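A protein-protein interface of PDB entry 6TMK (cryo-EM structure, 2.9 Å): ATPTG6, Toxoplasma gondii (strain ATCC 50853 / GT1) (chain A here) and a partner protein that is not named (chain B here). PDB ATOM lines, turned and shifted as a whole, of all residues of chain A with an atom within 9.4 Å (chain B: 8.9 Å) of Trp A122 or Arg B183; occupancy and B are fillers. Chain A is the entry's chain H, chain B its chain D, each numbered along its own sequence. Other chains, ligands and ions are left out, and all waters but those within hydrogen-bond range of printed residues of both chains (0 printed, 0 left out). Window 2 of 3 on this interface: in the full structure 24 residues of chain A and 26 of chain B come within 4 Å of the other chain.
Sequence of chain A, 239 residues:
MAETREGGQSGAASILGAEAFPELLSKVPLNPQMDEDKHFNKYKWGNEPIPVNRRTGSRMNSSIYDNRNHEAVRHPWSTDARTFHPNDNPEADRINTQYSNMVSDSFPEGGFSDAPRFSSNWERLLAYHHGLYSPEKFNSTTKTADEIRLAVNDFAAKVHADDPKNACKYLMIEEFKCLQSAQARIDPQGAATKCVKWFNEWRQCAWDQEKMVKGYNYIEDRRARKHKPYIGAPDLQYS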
ATOM      1  N   PRO A  76       3.537   6.985 -15.603  1.00  0.00           N
ATOM      2  CA  PRO A  76       3.736   5.545 -15.406  1.00  0.00           C
ATOM      3  C   PRO A  76       3.431   5.091 -13.994  1.00  0.00           C
ATOM      4  O   PRO A  76       3.016   3.942 -13.795  1.00  0.00           O
ATOM      5  CB  PRO A  76       5.215   5.347 -15.760  1.00  0.00           C
ATOM      6  CG  PRO A  76       5.572   6.496 -16.576  1.00  0.00           C
ATOM      7  CD  PRO A  76       4.758   7.639 -16.089  1.00  0.00           C
ATOM      8  N   TRP A  77       3.629   5.953 -13.009  1.00  0.00           N
ATOM      9  CA  TRP A  77       3.396   5.621 -11.617  1.00  0.00           C
ATOM     10  C   TRP A  77       1.991   6.031 -11.197  1.00  0.00           C
ATOM     11  O   TRP A  77       1.331   6.842 -11.848  1.00  0.00           O
ATOM     12  CB  TRP A  77       4.438   6.301 -10.729  1.00  0.00           C
ATOM     13  CG  TRP A  77       4.508   7.778 -10.879  1.00  0.00           C
ATOM     14  CD1 TRP A  77       3.795   8.703 -10.190  1.00  0.00           C
ATOM     15  CD2 TRP A  77       5.339   8.507 -11.784  1.00  0.00           C
ATOM     16  NE1 TRP A  77       4.128   9.964 -10.604  1.00  0.00           N
ATOM     17  CE2 TRP A  77       5.076   9.869 -11.584  1.00  0.00           C
ATOM     18  CE3 TRP A  77       6.284   8.139 -12.741  1.00  0.00           C
ATOM     19  CZ2 TRP A  77       5.723  10.861 -12.302  1.00  0.00           C
ATOM     20  CZ3 TRP A  77       6.915   9.121 -13.447  1.00  0.00           C
ATOM     21  CH2 TRP A  77       6.633  10.465 -13.229  1.00  0.00           C
ATOM     22  N   PHE A 118      10.251   5.783  -6.386  1.00  0.00           N
ATOM     23  CA  PHE A 118      10.534   4.612  -7.198  1.00  0.00           C
ATOM     24  C   PHE A 118      11.027   3.465  -6.329  1.00  0.00           C
ATOM     25  O   PHE A 118      11.876   3.653  -5.454  1.00  0.00           O
ATOM     26  CB  PHE A 118      11.586   4.953  -8.248  1.00  0.00           C
ATOM     27  CG  PHE A 118      11.065   5.733  -9.408  1.00  0.00           C
ATOM     28  CD1 PHE A 118      10.197   5.163 -10.310  1.00  0.00           C
ATOM     29  CD2 PHE A 118      11.452   7.040  -9.602  1.00  0.00           C
ATOM     30  CE1 PHE A 118       9.730   5.881 -11.375  1.00  0.00           C
ATOM     31  CE2 PHE A 118      10.983   7.756 -10.668  1.00  0.00           C
ATOM     32  CZ  PHE A 118      10.123   7.176 -11.554  1.00  0.00           C
ATOM     33  N   SER A 119      10.489   2.272  -6.578  1.00  0.00           N
ATOM     34  CA  SER A 119      10.911   1.080  -5.860  1.00  0.00           C
ATOM     35  C   SER A 119      12.281   0.592  -6.295  1.00  0.00           C
ATOM     36  O   SER A 119      12.861  -0.263  -5.619  1.00  0.00           O
ATOM     37  CB  SER A 119       9.889  -0.034  -6.068  1.00  0.00           C
ATOM     38  OG  SER A 119       8.604   0.358  -5.624  1.00  0.00           O
ATOM     39  N   SER A 120      12.808   1.117  -7.395  1.00  0.00           N
ATOM     40  CA  SER A 120      14.053   0.639  -7.968  1.00  0.00           C
ATOM     41  C   SER A 120      14.693   1.777  -8.747  1.00  0.00           C
ATOM     42  O   SER A 120      14.056   2.789  -9.047  1.00  0.00           O
ATOM     43  CB  SER A 120      13.811  -0.578  -8.861  1.00  0.00           C
ATOM     44  OG  SER A 120      13.273  -1.648  -8.106  1.00  0.00           O
ATOM     45  N   ASN A 121      15.972   1.601  -9.073  1.00  0.00           N
ATOM     46  CA  ASN A 121      16.685   2.602  -9.852  1.00  0.00           C
ATOM     47  C   ASN A 121      16.426   2.457 -11.346  1.00  0.00           C
ATOM     48  O   ASN A 121      16.470   3.452 -12.081  1.00  0.00           O
ATOM     49  CB  ASN A 121      18.179   2.512  -9.558  1.00  0.00           C
ATOM     50  CG  ASN A 121      18.980   3.558 -10.297  1.00  0.00           C
ATOM     51  OD1 ASN A 121      18.555   4.704 -10.437  1.00  0.00           O
ATOM     52  ND2 ASN A 121      20.148   3.166 -10.782  1.00  0.00           N
ATOM     53  N   TRP A 122      16.147   1.243 -11.814  1.00  0.00           N
ATOM     54  CA  TRP A 122      15.958   1.042 -13.242  1.00  0.00           C
ATOM     55  C   TRP A 122      14.622   1.597 -13.710  1.00  0.00           C
ATOM     56  O   TRP A 122      14.495   2.003 -14.868  1.00  0.00           O
ATOM     57  CB  TRP A 122      16.097  -0.436 -13.599  1.00  0.00           C
ATOM     58  CG  TRP A 122      15.096  -1.350 -12.992  1.00  0.00           C
ATOM     59  CD1 TRP A 122      15.214  -2.024 -11.819  1.00  0.00           C
ATOM     60  CD2 TRP A 122      13.832  -1.723 -13.543  1.00  0.00           C
ATOM     61  NE1 TRP A 122      14.099  -2.784 -11.597  1.00  0.00           N
ATOM     62  CE2 TRP A 122      13.234  -2.615 -12.641  1.00  0.00           C
ATOM     63  CE3 TRP A 122      13.143  -1.382 -14.708  1.00  0.00           C
ATOM     64  CZ2 TRP A 122      11.987  -3.167 -12.864  1.00  0.00           C
ATOM     65  CZ3 TRP A 122      11.907  -1.932 -14.924  1.00  0.00           C
ATOM     66  CH2 TRP A 122      11.340  -2.814 -14.012  1.00  0.00           C
ATOM     67  N   GLU A 123      13.627   1.657 -12.827  1.00  0.00           N
ATOM     68  CA  GLU A 123      12.376   2.324 -13.166  1.00  0.00           C
ATOM     69  C   GLU A 123      12.605   3.812 -13.387  1.00  0.00           C
ATOM     70  O   GLU A 123      12.085   4.404 -14.339  1.00  0.00           O
ATOM     71  CB  GLU A 123      11.362   2.096 -12.053  1.00  0.00           C
ATOM     72  CG  GLU A 123      10.893   0.674 -11.941  1.00  0.00           C
ATOM     73  CD  GLU A 123      10.235   0.377 -10.612  1.00  0.00           C
ATOM     74  OE1 GLU A 123       9.801   1.331  -9.931  1.00  0.00           O
ATOM     75  OE2 GLU A 123      10.157  -0.812 -10.239  1.00  0.00           O
ATOM     76  N   ARG A 124      13.365   4.432 -12.490  1.00  0.00           N
ATOM     77  CA  ARG A 124      13.767   5.822 -12.652  1.00  0.00           C
ATOM     78  C   ARG A 124      14.482   6.025 -13.979  1.00  0.00           C
ATOM     79  O   ARG A 124      14.164   6.946 -14.747  1.00  0.00           O
ATOM     80  CB  ARG A 124      14.668   6.197 -11.483  1.00  0.00           C
ATOM     81  CG  ARG A 124      14.930   7.656 -11.276  1.00  0.00           C
ATOM     82  CD  ARG A 124      15.947   7.834 -10.170  1.00  0.00           C
ATOM     83  NE  ARG A 124      15.386   7.543  -8.858  1.00  0.00           N
ATOM     84  CZ  ARG A 124      14.736   8.423  -8.108  1.00  0.00           C
ATOM     85  NH1 ARG A 124      14.559   9.664  -8.531  1.00  0.00           N
ATOM     86  NH2 ARG A 124      14.261   8.058  -6.930  1.00  0.00           N
ATOM     87  N   LEU A 125      15.461   5.168 -14.257  1.00  0.00           N
ATOM     88  CA  LEU A 125      16.200   5.238 -15.509  1.00  0.00           C
ATOM     89  C   LEU A 125      15.273   5.162 -16.711  1.00  0.00           C
ATOM     90  O   LEU A 125      15.399   5.946 -17.652  1.00  0.00           O
ATOM     91  CB  LEU A 125      17.221   4.111 -15.559  1.00  0.00           C
ATOM     92  CG  LEU A 125      18.590   4.423 -14.991  1.00  0.00           C
ATOM     93  CD1 LEU A 125      19.310   3.139 -14.686  1.00  0.00           C
ATOM     94  CD2 LEU A 125      19.345   5.241 -16.007  1.00  0.00           C
ATOM     95  N   LEU A 126      14.353   4.202 -16.710  1.00  0.00           N
ATOM     96  CA  LEU A 126      13.490   3.999 -17.862  1.00  0.00           C
ATOM     97  C   LEU A 126      12.539   5.169 -18.061  1.00  0.00           C
ATOM     98  O   LEU A 126      12.306   5.604 -19.197  1.00  0.00           O
ATOM     99  CB  LEU A 126      12.723   2.695 -17.695  1.00  0.00           C
ATOM    100  CG  LEU A 126      12.159   2.077 -18.966  1.00  0.00           C
ATOM    101  CD1 LEU A 126      13.247   1.583 -19.873  1.00  0.00           C
ATOM    102  CD2 LEU A 126      11.247   0.965 -18.588  1.00  0.00           C
ATOM    103  N   ALA A 127      11.982   5.692 -16.972  1.00  0.00           N
ATOM    104  CA  ALA A 127      11.112   6.855 -17.073  1.00  0.00           C
ATOM    105  C   ALA A 127      11.857   8.043 -17.661  1.00  0.00           C
ATOM    106  O   ALA A 127      11.359   8.719 -18.571  1.00  0.00           O
ATOM    107  CB  ALA A 127      10.551   7.196 -15.701  1.00  0.00           C
ATOM    108  N   TYR A 128      13.066   8.309 -17.162  1.00  0.00           N
ATOM    109  CA  TYR A 128      13.863   9.388 -17.727  1.00  0.00           C
ATOM    110  C   TYR A 128      14.171   9.138 -19.197  1.00  0.00           C
ATOM    111  O   TYR A 128      14.054  10.043 -20.030  1.00  0.00           O
ATOM    112  CB  TYR A 128      15.160   9.545 -16.942  1.00  0.00           C
ATOM    113  CG  TYR A 128      16.100  10.542 -17.568  1.00  0.00           C
ATOM    114  CD1 TYR A 128      15.857  11.897 -17.484  1.00  0.00           C
ATOM    115  CD2 TYR A 128      17.209  10.123 -18.277  1.00  0.00           C
ATOM    116  CE1 TYR A 128      16.699  12.803 -18.065  1.00  0.00           C
ATOM    117  CE2 TYR A 128      18.053  11.020 -18.862  1.00  0.00           C
ATOM    118  CZ  TYR A 128      17.795  12.362 -18.757  1.00  0.00           C
ATOM    119  OH  TYR A 128      18.642  13.268 -19.346  1.00  0.00           O
ATOM    120  N   HIS A 129      14.554   7.910 -19.529  1.00  0.00           N
ATOM    121  CA  HIS A 129      14.929   7.572 -20.891  1.00  0.00           C
ATOM    122  C   HIS A 129      13.775   7.775 -21.857  1.00  0.00           C
ATOM    123  O   HIS A 129      13.994   8.129 -23.019  1.00  0.00           O
ATOM    124  CB  HIS A 129      15.425   6.130 -20.925  1.00  0.00           C
ATOM    125  CG  HIS A 129      15.626   5.587 -22.299  1.00  0.00           C
ATOM    126  ND1 HIS A 129      16.707   5.927 -23.079  1.00  0.00           N
ATOM    127  CD2 HIS A 129      14.883   4.732 -23.036  1.00  0.00           C
ATOM    128  CE1 HIS A 129      16.627   5.296 -24.234  1.00  0.00           C
ATOM    129  NE2 HIS A 129      15.528   4.567 -24.235  1.00  0.00           N
ATOM    130  N   HIS A 130      12.549   7.558 -21.406  1.00  0.00           N
ATOM    131  CA  HIS A 130      11.391   7.743 -22.263  1.00  0.00           C
ATOM    132  C   HIS A 130      10.769   9.124 -22.143  1.00  0.00           C
ATOM    133  O   HIS A 130       9.809   9.417 -22.861  1.00  0.00           O
ATOM    134  CB  HIS A 130      10.344   6.679 -21.970  1.00  0.00           C
ATOM    135  CG  HIS A 130      10.608   5.387 -22.667  1.00  0.00           C
ATOM    136  ND1 HIS A 130      10.435   5.229 -24.023  1.00  0.00           N
ATOM    137  CD2 HIS A 130      11.067   4.206 -22.204  1.00  0.00           C
ATOM    138  CE1 HIS A 130      10.761   3.997 -24.361  1.00  0.00           C
ATOM    139  NE2 HIS A 130      11.144   3.355 -23.275  1.00  0.00           N
ATOM    140  N   TYR A 133      10.034  11.618 -16.666  1.00  0.00           N
ATOM    141  CA  TYR A 133      10.479  11.972 -15.329  1.00  0.00           C
ATOM    142  C   TYR A 133      11.712  12.851 -15.414  1.00  0.00           C
ATOM    143  O   TYR A 133      12.644  12.547 -16.160  1.00  0.00           O
ATOM    144  CB  TYR A 133      10.784  10.728 -14.499  1.00  0.00           C
ATOM    145  CG  TYR A 133      11.538  11.022 -13.238  1.00  0.00           C
ATOM    146  CD1 TYR A 133      10.909  11.600 -12.156  1.00  0.00           C
ATOM    147  CD2 TYR A 133      12.879  10.725 -13.130  1.00  0.00           C
ATOM    148  CE1 TYR A 133      11.593  11.870 -11.006  1.00  0.00           C
ATOM    149  CE2 TYR A 133      13.571  10.993 -11.985  1.00  0.00           C
ATOM    150  CZ  TYR A 133      12.924  11.566 -10.922  1.00  0.00           C
ATOM    151  OH  TYR A 133      13.610  11.839  -9.766  1.00  0.00           O
ATOM    152  N   LEU B 176       3.991   6.836 -22.944  1.00  0.00           N
ATOM    153  CA  LEU B 176       3.689   5.757 -22.014  1.00  0.00           C
ATOM    154  C   LEU B 176       3.643   4.407 -22.713  1.00  0.00           C
ATOM    155  O   LEU B 176       4.056   3.390 -22.147  1.00  0.00           O
ATOM    156  CB  LEU B 176       2.353   6.036 -21.340  1.00  0.00           C
ATOM    157  CG  LEU B 176       2.281   7.267 -20.451  1.00  0.00           C
ATOM    158  CD1 LEU B 176       0.848   7.643 -20.191  1.00  0.00           C
ATOM    159  CD2 LEU B 176       2.983   7.017 -19.165  1.00  0.00           C
ATOM    160  N   GLN B 177       3.128   4.374 -23.939  1.00  0.00           N
ATOM    161  CA  GLN B 177       3.046   3.130 -24.689  1.00  0.00           C
ATOM    162  C   GLN B 177       4.437   2.581 -24.974  1.00  0.00           C
ATOM    163  O   GLN B 177       4.702   1.384 -24.795  1.00  0.00           O
ATOM    164  CB  GLN B 177       2.268   3.380 -25.977  1.00  0.00           C
ATOM    165  CG  GLN B 177       2.071   2.187 -26.866  1.00  0.00           C
ATOM    166  CD  GLN B 177       1.420   1.034 -26.150  1.00  0.00           C
ATOM    167  OE1 GLN B 177       0.651   1.223 -25.215  1.00  0.00           O
ATOM    168  NE2 GLN B 177       1.717  -0.169 -26.592  1.00  0.00           N
ATOM    169  N   ARG B 178       5.342   3.450 -25.425  1.00  0.00           N
ATOM    170  CA  ARG B 178       6.723   3.032 -25.635  1.00  0.00           C
ATOM    171  C   ARG B 178       7.345   2.533 -24.341  1.00  0.00           C
ATOM    172  O   ARG B 178       8.026   1.500 -24.318  1.00  0.00           O
ATOM    173  CB  ARG B 178       7.536   4.186 -26.192  1.00  0.00           C
ATOM    174  CG  ARG B 178       7.309   4.476 -27.623  1.00  0.00           C
ATOM    175  CD  ARG B 178       8.459   5.266 -28.150  1.00  0.00           C
ATOM    176  NE  ARG B 178       8.572   6.554 -27.476  1.00  0.00           N
ATOM    177  CZ  ARG B 178       7.953   7.663 -27.868  1.00  0.00           C
ATOM    178  NH1 ARG B 178       7.160   7.657 -28.928  1.00  0.00           N
ATOM    179  NH2 ARG B 178       8.125   8.781 -27.186  1.00  0.00           N
ATOM    180  N   HIS B 179       7.138   3.276 -23.256  1.00  0.00           N
ATOM    181  CA  HIS B 179       7.664   2.879 -21.959  1.00  0.00           C
ATOM    182  C   HIS B 179       7.199   1.482 -21.573  1.00  0.00           C
ATOM    183  O   HIS B 179       7.998   0.646 -21.138  1.00  0.00           O
ATOM    184  CB  HIS B 179       7.235   3.914 -20.927  1.00  0.00           C
ATOM    185  CG  HIS B 179       7.604   3.575 -19.521  1.00  0.00           C
ATOM    186  ND1 HIS B 179       8.788   3.974 -18.945  1.00  0.00           N
ATOM    187  CD2 HIS B 179       6.923   2.909 -18.563  1.00  0.00           C
ATOM    188  CE1 HIS B 179       8.828   3.547 -17.698  1.00  0.00           C
ATOM    189  NE2 HIS B 179       7.711   2.897 -17.442  1.00  0.00           N
ATOM    190  N   ALA B 180       5.907   1.207 -21.737  1.00  0.00           N
ATOM    191  CA  ALA B 180       5.361  -0.077 -21.320  1.00  0.00           C
ATOM    192  C   ALA B 180       5.880  -1.214 -22.190  1.00  0.00           C
ATOM    193  O   ALA B 180       6.236  -2.281 -21.677  1.00  0.00           O
ATOM    194  CB  ALA B 180       3.841  -0.020 -21.350  1.00  0.00           C
ATOM    195  N   GLU B 181       5.927  -1.011 -23.507  1.00  0.00           N
ATOM    196  CA  GLU B 181       6.476  -2.036 -24.386  1.00  0.00           C
ATOM    197  C   GLU B 181       7.917  -2.363 -24.019  1.00  0.00           C
ATOM    198  O   GLU B 181       8.306  -3.537 -23.943  1.00  0.00           O
ATOM    199  CB  GLU B 181       6.384  -1.579 -25.836  1.00  0.00           C
ATOM    200  CG  GLU B 181       4.980  -1.494 -26.358  1.00  0.00           C
ATOM    201  CD  GLU B 181       4.924  -0.949 -27.769  1.00  0.00           C
ATOM    202  OE1 GLU B 181       5.937  -1.069 -28.489  1.00  0.00           O
ATOM    203  OE2 GLU B 181       3.873  -0.400 -28.161  1.00  0.00           O
ATOM    204  N   HIS B 182       8.728  -1.331 -23.792  1.00  0.00           N
ATOM    205  CA  HIS B 182      10.129  -1.537 -23.451  1.00  0.00           C
ATOM    206  C   HIS B 182      10.266  -2.274 -22.122  1.00  0.00           C
ATOM    207  O   HIS B 182      11.059  -3.215 -21.996  1.00  0.00           O
ATOM    208  CB  HIS B 182      10.829  -0.182 -23.409  1.00  0.00           C
ATOM    209  CG  HIS B 182      12.319  -0.257 -23.450  1.00  0.00           C
ATOM    210  ND1 HIS B 182      13.118   0.835 -23.198  1.00  0.00           N
ATOM    211  CD2 HIS B 182      13.158  -1.283 -23.720  1.00  0.00           C
ATOM    212  CE1 HIS B 182      14.385   0.484 -23.303  1.00  0.00           C
ATOM    213  NE2 HIS B 182      14.436  -0.796 -23.619  1.00  0.00           N
ATOM    214  N   ARG B 183       9.494  -1.854 -21.120  1.00  0.00           N
ATOM    215  CA  ARG B 183       9.510  -2.513 -19.820  1.00  0.00           C
ATOM    216  C   ARG B 183       9.157  -3.990 -19.933  1.00  0.00           C
ATOM    217  O   ARG B 183       9.798  -4.842 -19.304  1.00  0.00           O
ATOM    218  CB  ARG B 183       8.536  -1.798 -18.890  1.00  0.00           C
ATOM    219  CG  ARG B 183       8.705  -2.100 -17.435  1.00  0.00           C
ATOM    220  CD  ARG B 183       7.438  -1.791 -16.693  1.00  0.00           C
ATOM    221  NE  ARG B 183       7.489  -2.214 -15.297  1.00  0.00           N
ATOM    222  CZ  ARG B 183       7.758  -1.412 -14.275  1.00  0.00           C
ATOM    223  NH1 ARG B 183       8.014  -0.125 -14.469  1.00  0.00           N
ATOM    224  NH2 ARG B 183       7.777  -1.901 -13.049  1.00  0.00           N
ATOM    225  N   ASN B 184       8.141  -4.313 -20.730  1.00  0.00           N
ATOM    226  CA  ASN B 184       7.710  -5.700 -20.858  1.00  0.00           C
ATOM    227  C   ASN B 184       8.764  -6.538 -21.567  1.00  0.00           C
ATOM    228  O   ASN B 184       9.070  -7.659 -21.139  1.00  0.00           O
ATOM    229  CB  ASN B 184       6.382  -5.756 -21.606  1.00  0.00           C
ATOM    230  CG  ASN B 184       5.214  -5.332 -20.749  1.00  0.00           C
ATOM    231  OD1 ASN B 184       5.237  -5.480 -19.529  1.00  0.00           O
ATOM    232  ND2 ASN B 184       4.187  -4.786 -21.383  1.00  0.00           N
ATOM    233  N   ASP B 185       9.318  -6.017 -22.662  1.00  0.00           N
ATOM    234  CA  ASP B 185      10.443  -6.677 -23.314  1.00  0.00           C
ATOM    235  C   ASP B 185      11.549  -6.983 -22.311  1.00  0.00           C
ATOM    236  O   ASP B 185      12.071  -8.104 -22.258  1.00  0.00           O
ATOM    237  CB  ASP B 185      10.970  -5.801 -24.447  1.00  0.00           C
ATOM    238  CG  ASP B 185      10.157  -5.932 -25.718  1.00  0.00           C
ATOM    239  OD1 ASP B 185       9.403  -6.919 -25.855  1.00  0.00           O
ATOM    240  OD2 ASP B 185      10.270  -5.039 -26.585  1.00  0.00           O
ATOM    241  N   LEU B 186      11.907  -5.994 -21.492  1.00  0.00           N
ATOM    242  CA  LEU B 186      13.027  -6.155 -20.574  1.00  0.00           C
ATOM    243  C   LEU B 186      12.736  -7.233 -19.540  1.00  0.00           C
ATOM    244  O   LEU B 186      13.585  -8.084 -19.255  1.00  0.00           O
ATOM    245  CB  LEU B 186      13.338  -4.829 -19.887  1.00  0.00           C
ATOM    246  CG  LEU B 186      13.924  -3.720 -20.748  1.00  0.00           C
ATOM    247  CD1 LEU B 186      13.692  -2.380 -20.102  1.00  0.00           C
ATOM    248  CD2 LEU B 186      15.391  -3.955 -20.957  1.00  0.00           C
ATOM    249  N   GLU B 187      11.542  -7.207 -18.954  1.00  0.00           N
ATOM    250  CA  GLU B 187      11.229  -8.150 -17.890  1.00  0.00           C
ATOM    251  C   GLU B 187      11.115  -9.572 -18.430  1.00  0.00           C
ATOM    252  O   GLU B 187      11.554 -10.531 -17.780  1.00  0.00           O
ATOM    253  CB  GLU B 187       9.946  -7.723 -17.191  1.00  0.00           C
ATOM    254  CG  GLU B 187      10.118  -6.479 -16.356  1.00  0.00           C
ATOM    255  CD  GLU B 187       8.850  -6.046 -15.655  1.00  0.00           C
ATOM    256  OE1 GLU B 187       8.841  -6.018 -14.407  1.00  0.00           O
ATOM    257  OE2 GLU B 187       7.863  -5.729 -16.349  1.00  0.00           O
ATOM    258  N   THR B 188      10.548  -9.728 -19.625  1.00  0.00           N
ATOM    259  CA  THR B 188      10.501 -11.043 -20.252  1.00  0.00           C
ATOM    260  C   THR B 188      11.904 -11.571 -20.534  1.00  0.00           C
ATOM    261  O   THR B 188      12.205 -12.745 -20.267  1.00  0.00           O
ATOM    262  CB  THR B 188       9.682 -10.957 -21.535  1.00  0.00           C
ATOM    263  OG1 THR B 188       8.306 -10.749 -21.205  1.00  0.00           O
ATOM    264  CG2 THR B 188       9.815 -12.211 -22.346  1.00  0.00           C
ATOM    265  N   THR B 189      12.777 -10.718 -21.073  1.00  0.00           N
ATOM    266  CA  THR B 189      14.150 -11.130 -21.325  1.00  0.00           C
ATOM    267  C   THR B 189      14.862 -11.497 -20.032  1.00  0.00           C
ATOM    268  O   THR B 189      15.677 -12.423 -20.009  1.00  0.00           O
ATOM    269  CB  THR B 189      14.894 -10.024 -22.063  1.00  0.00           C
ATOM    270  OG1 THR B 189      14.192  -9.704 -23.265  1.00  0.00           O
ATOM    271  CG2 THR B 189      16.287 -10.455 -22.404  1.00  0.00           C
ATOM    272  N   TRP B 190      14.555 -10.799 -18.941  1.00  0.00           N
ATOM    273  CA  TRP B 190      15.174 -11.127 -17.662  1.00  0.00           C
ATOM    274  C   TRP B 190      14.724 -12.490 -17.167  1.00  0.00           C
ATOM    275  O   TRP B 190      15.536 -13.271 -16.663  1.00  0.00           O
ATOM    276  CB  TRP B 190      14.851 -10.068 -16.617  1.00  0.00           C
ATOM    277  CG  TRP B 190      15.015 -10.580 -15.231  1.00  0.00           C
ATOM    278  CD1 TRP B 190      14.029 -10.844 -14.339  1.00  0.00           C
ATOM    279  CD2 TRP B 190      16.242 -10.905 -14.581  1.00  0.00           C
ATOM    280  NE1 TRP B 190      14.563 -11.317 -13.171  1.00  0.00           N
ATOM    281  CE2 TRP B 190      15.924 -11.361 -13.295  1.00  0.00           C
ATOM    282  CE3 TRP B 190      17.579 -10.856 -14.962  1.00  0.00           C
ATOM    283  CZ2 TRP B 190      16.892 -11.758 -12.391  1.00  0.00           C
ATOM    284  CZ3 TRP B 190      18.530 -11.249 -14.066  1.00  0.00           C
ATOM    285  CH2 TRP B 190      18.187 -11.695 -12.797  1.00  0.00           C
ATOM    286  N   GLU B 191      13.433 -12.784 -17.278  1.00  0.00           N
ATOM    287  CA  GLU B 191      12.946 -14.097 -16.872  1.00  0.00           C
ATOM    288  C   GLU B 191      13.630 -15.201 -17.669  1.00  0.00           C
ATOM    289  O   GLU B 191      14.115 -16.190 -17.100  1.00  0.00           O
ATOM    290  CB  GLU B 191      11.434 -14.158 -17.052  1.00  0.00           C
ATOM    291  CG  GLU B 191      10.679 -13.285 -16.097  1.00  0.00           C
ATOM    292  CD  GLU B 191       9.221 -13.138 -16.478  1.00  0.00           C
ATOM    293  OE1 GLU B 191       8.797 -13.774 -17.465  1.00  0.00           O
ATOM    294  OE2 GLU B 191       8.496 -12.383 -15.795  1.00  0.00           O
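A ring nitrogen (NE2) of His A130 lies within hydrogen-bond range of a ring nitrogen (ND1) of His B182 (3.2 Å).
NH2 of Arg B183 is in salt-bridge range of OE2 of Glu A123 (3.8 Å).
The guanidinium group (NE) of Arg B183 is in salt-bridge range of the side-chain carboxylate (OE2) of Glu B187, at 3.7 Å.
Leu B176 touches Pro A76.
Pro A76 touches His B179.
Trp A122 touches Arg B183 (CH2 to NH2, 3.8 Å).
His B179 touches Leu A126 (CE1 to CD2, 3.6 Å).
Leu A126 touches His B182 (CD1 to ND1, 3.4 Å).
Leu A126 touches Arg B183.
Leu B186 touches Leu A126 (CD1 to CD1, 3.99 Å).
His B179 touches Ala A127 (CE1 to N, 3.9 Å).
His A130 touches Arg B178 (CE1 to O, 3.7 Å).
His B179 touches His A130 (CA to CD2, 3.7 Å).
Of chain B, only Arg B183 comes within 4 Å of Trp A122.
Of chain A, only Trp A122 (3.8 Å), Glu A123 (3.8 Å) and Leu A126 (3.9 Å) come within 4 Å of Arg B183.
No residue of chain B comes within 4 Å of Asn A121.
No residue of chain A comes within 4 Å of Asn B184.
Of the printed residues of chain A, Leu B186 touches Leu A126 (3.99 Å).
Printed residues of chain B within 4 Å of Leu A126: His B179, His B182, Arg B183 and Leu B186.
Printed residues of chain B within 4 Å of Glu A123: Arg B183.
Of the printed residues of chain B, Pro A76 touches Leu B176 (3.6 Å) and His B179 (3.9 Å).
Trp B190 touches none of the printed residues of chain A.
The nearest residue of chain A that does not touch Arg B183 is His A130 (5.9 Å).
Printed residues of chain B that touch a printed residue of chain A: Leu B176, Arg B178, His B179, His B182, Arg B183 and Leu B186.
Hydrophobic or aromatic side chains of chain B within 4 Å of the printed part of chain A: Leu B176, His B179, His B182 and Leu B186.
Of the 16 printed residues of chain A, 6 touch a printed residue of chain B.
Printed residues of chain A that touch a printed residue of chain B: Pro A76, Trp A122, Glu A123, Leu A126, Ala A127 and His A130.
Among the printed residues, 12 pairs touch across the chains.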
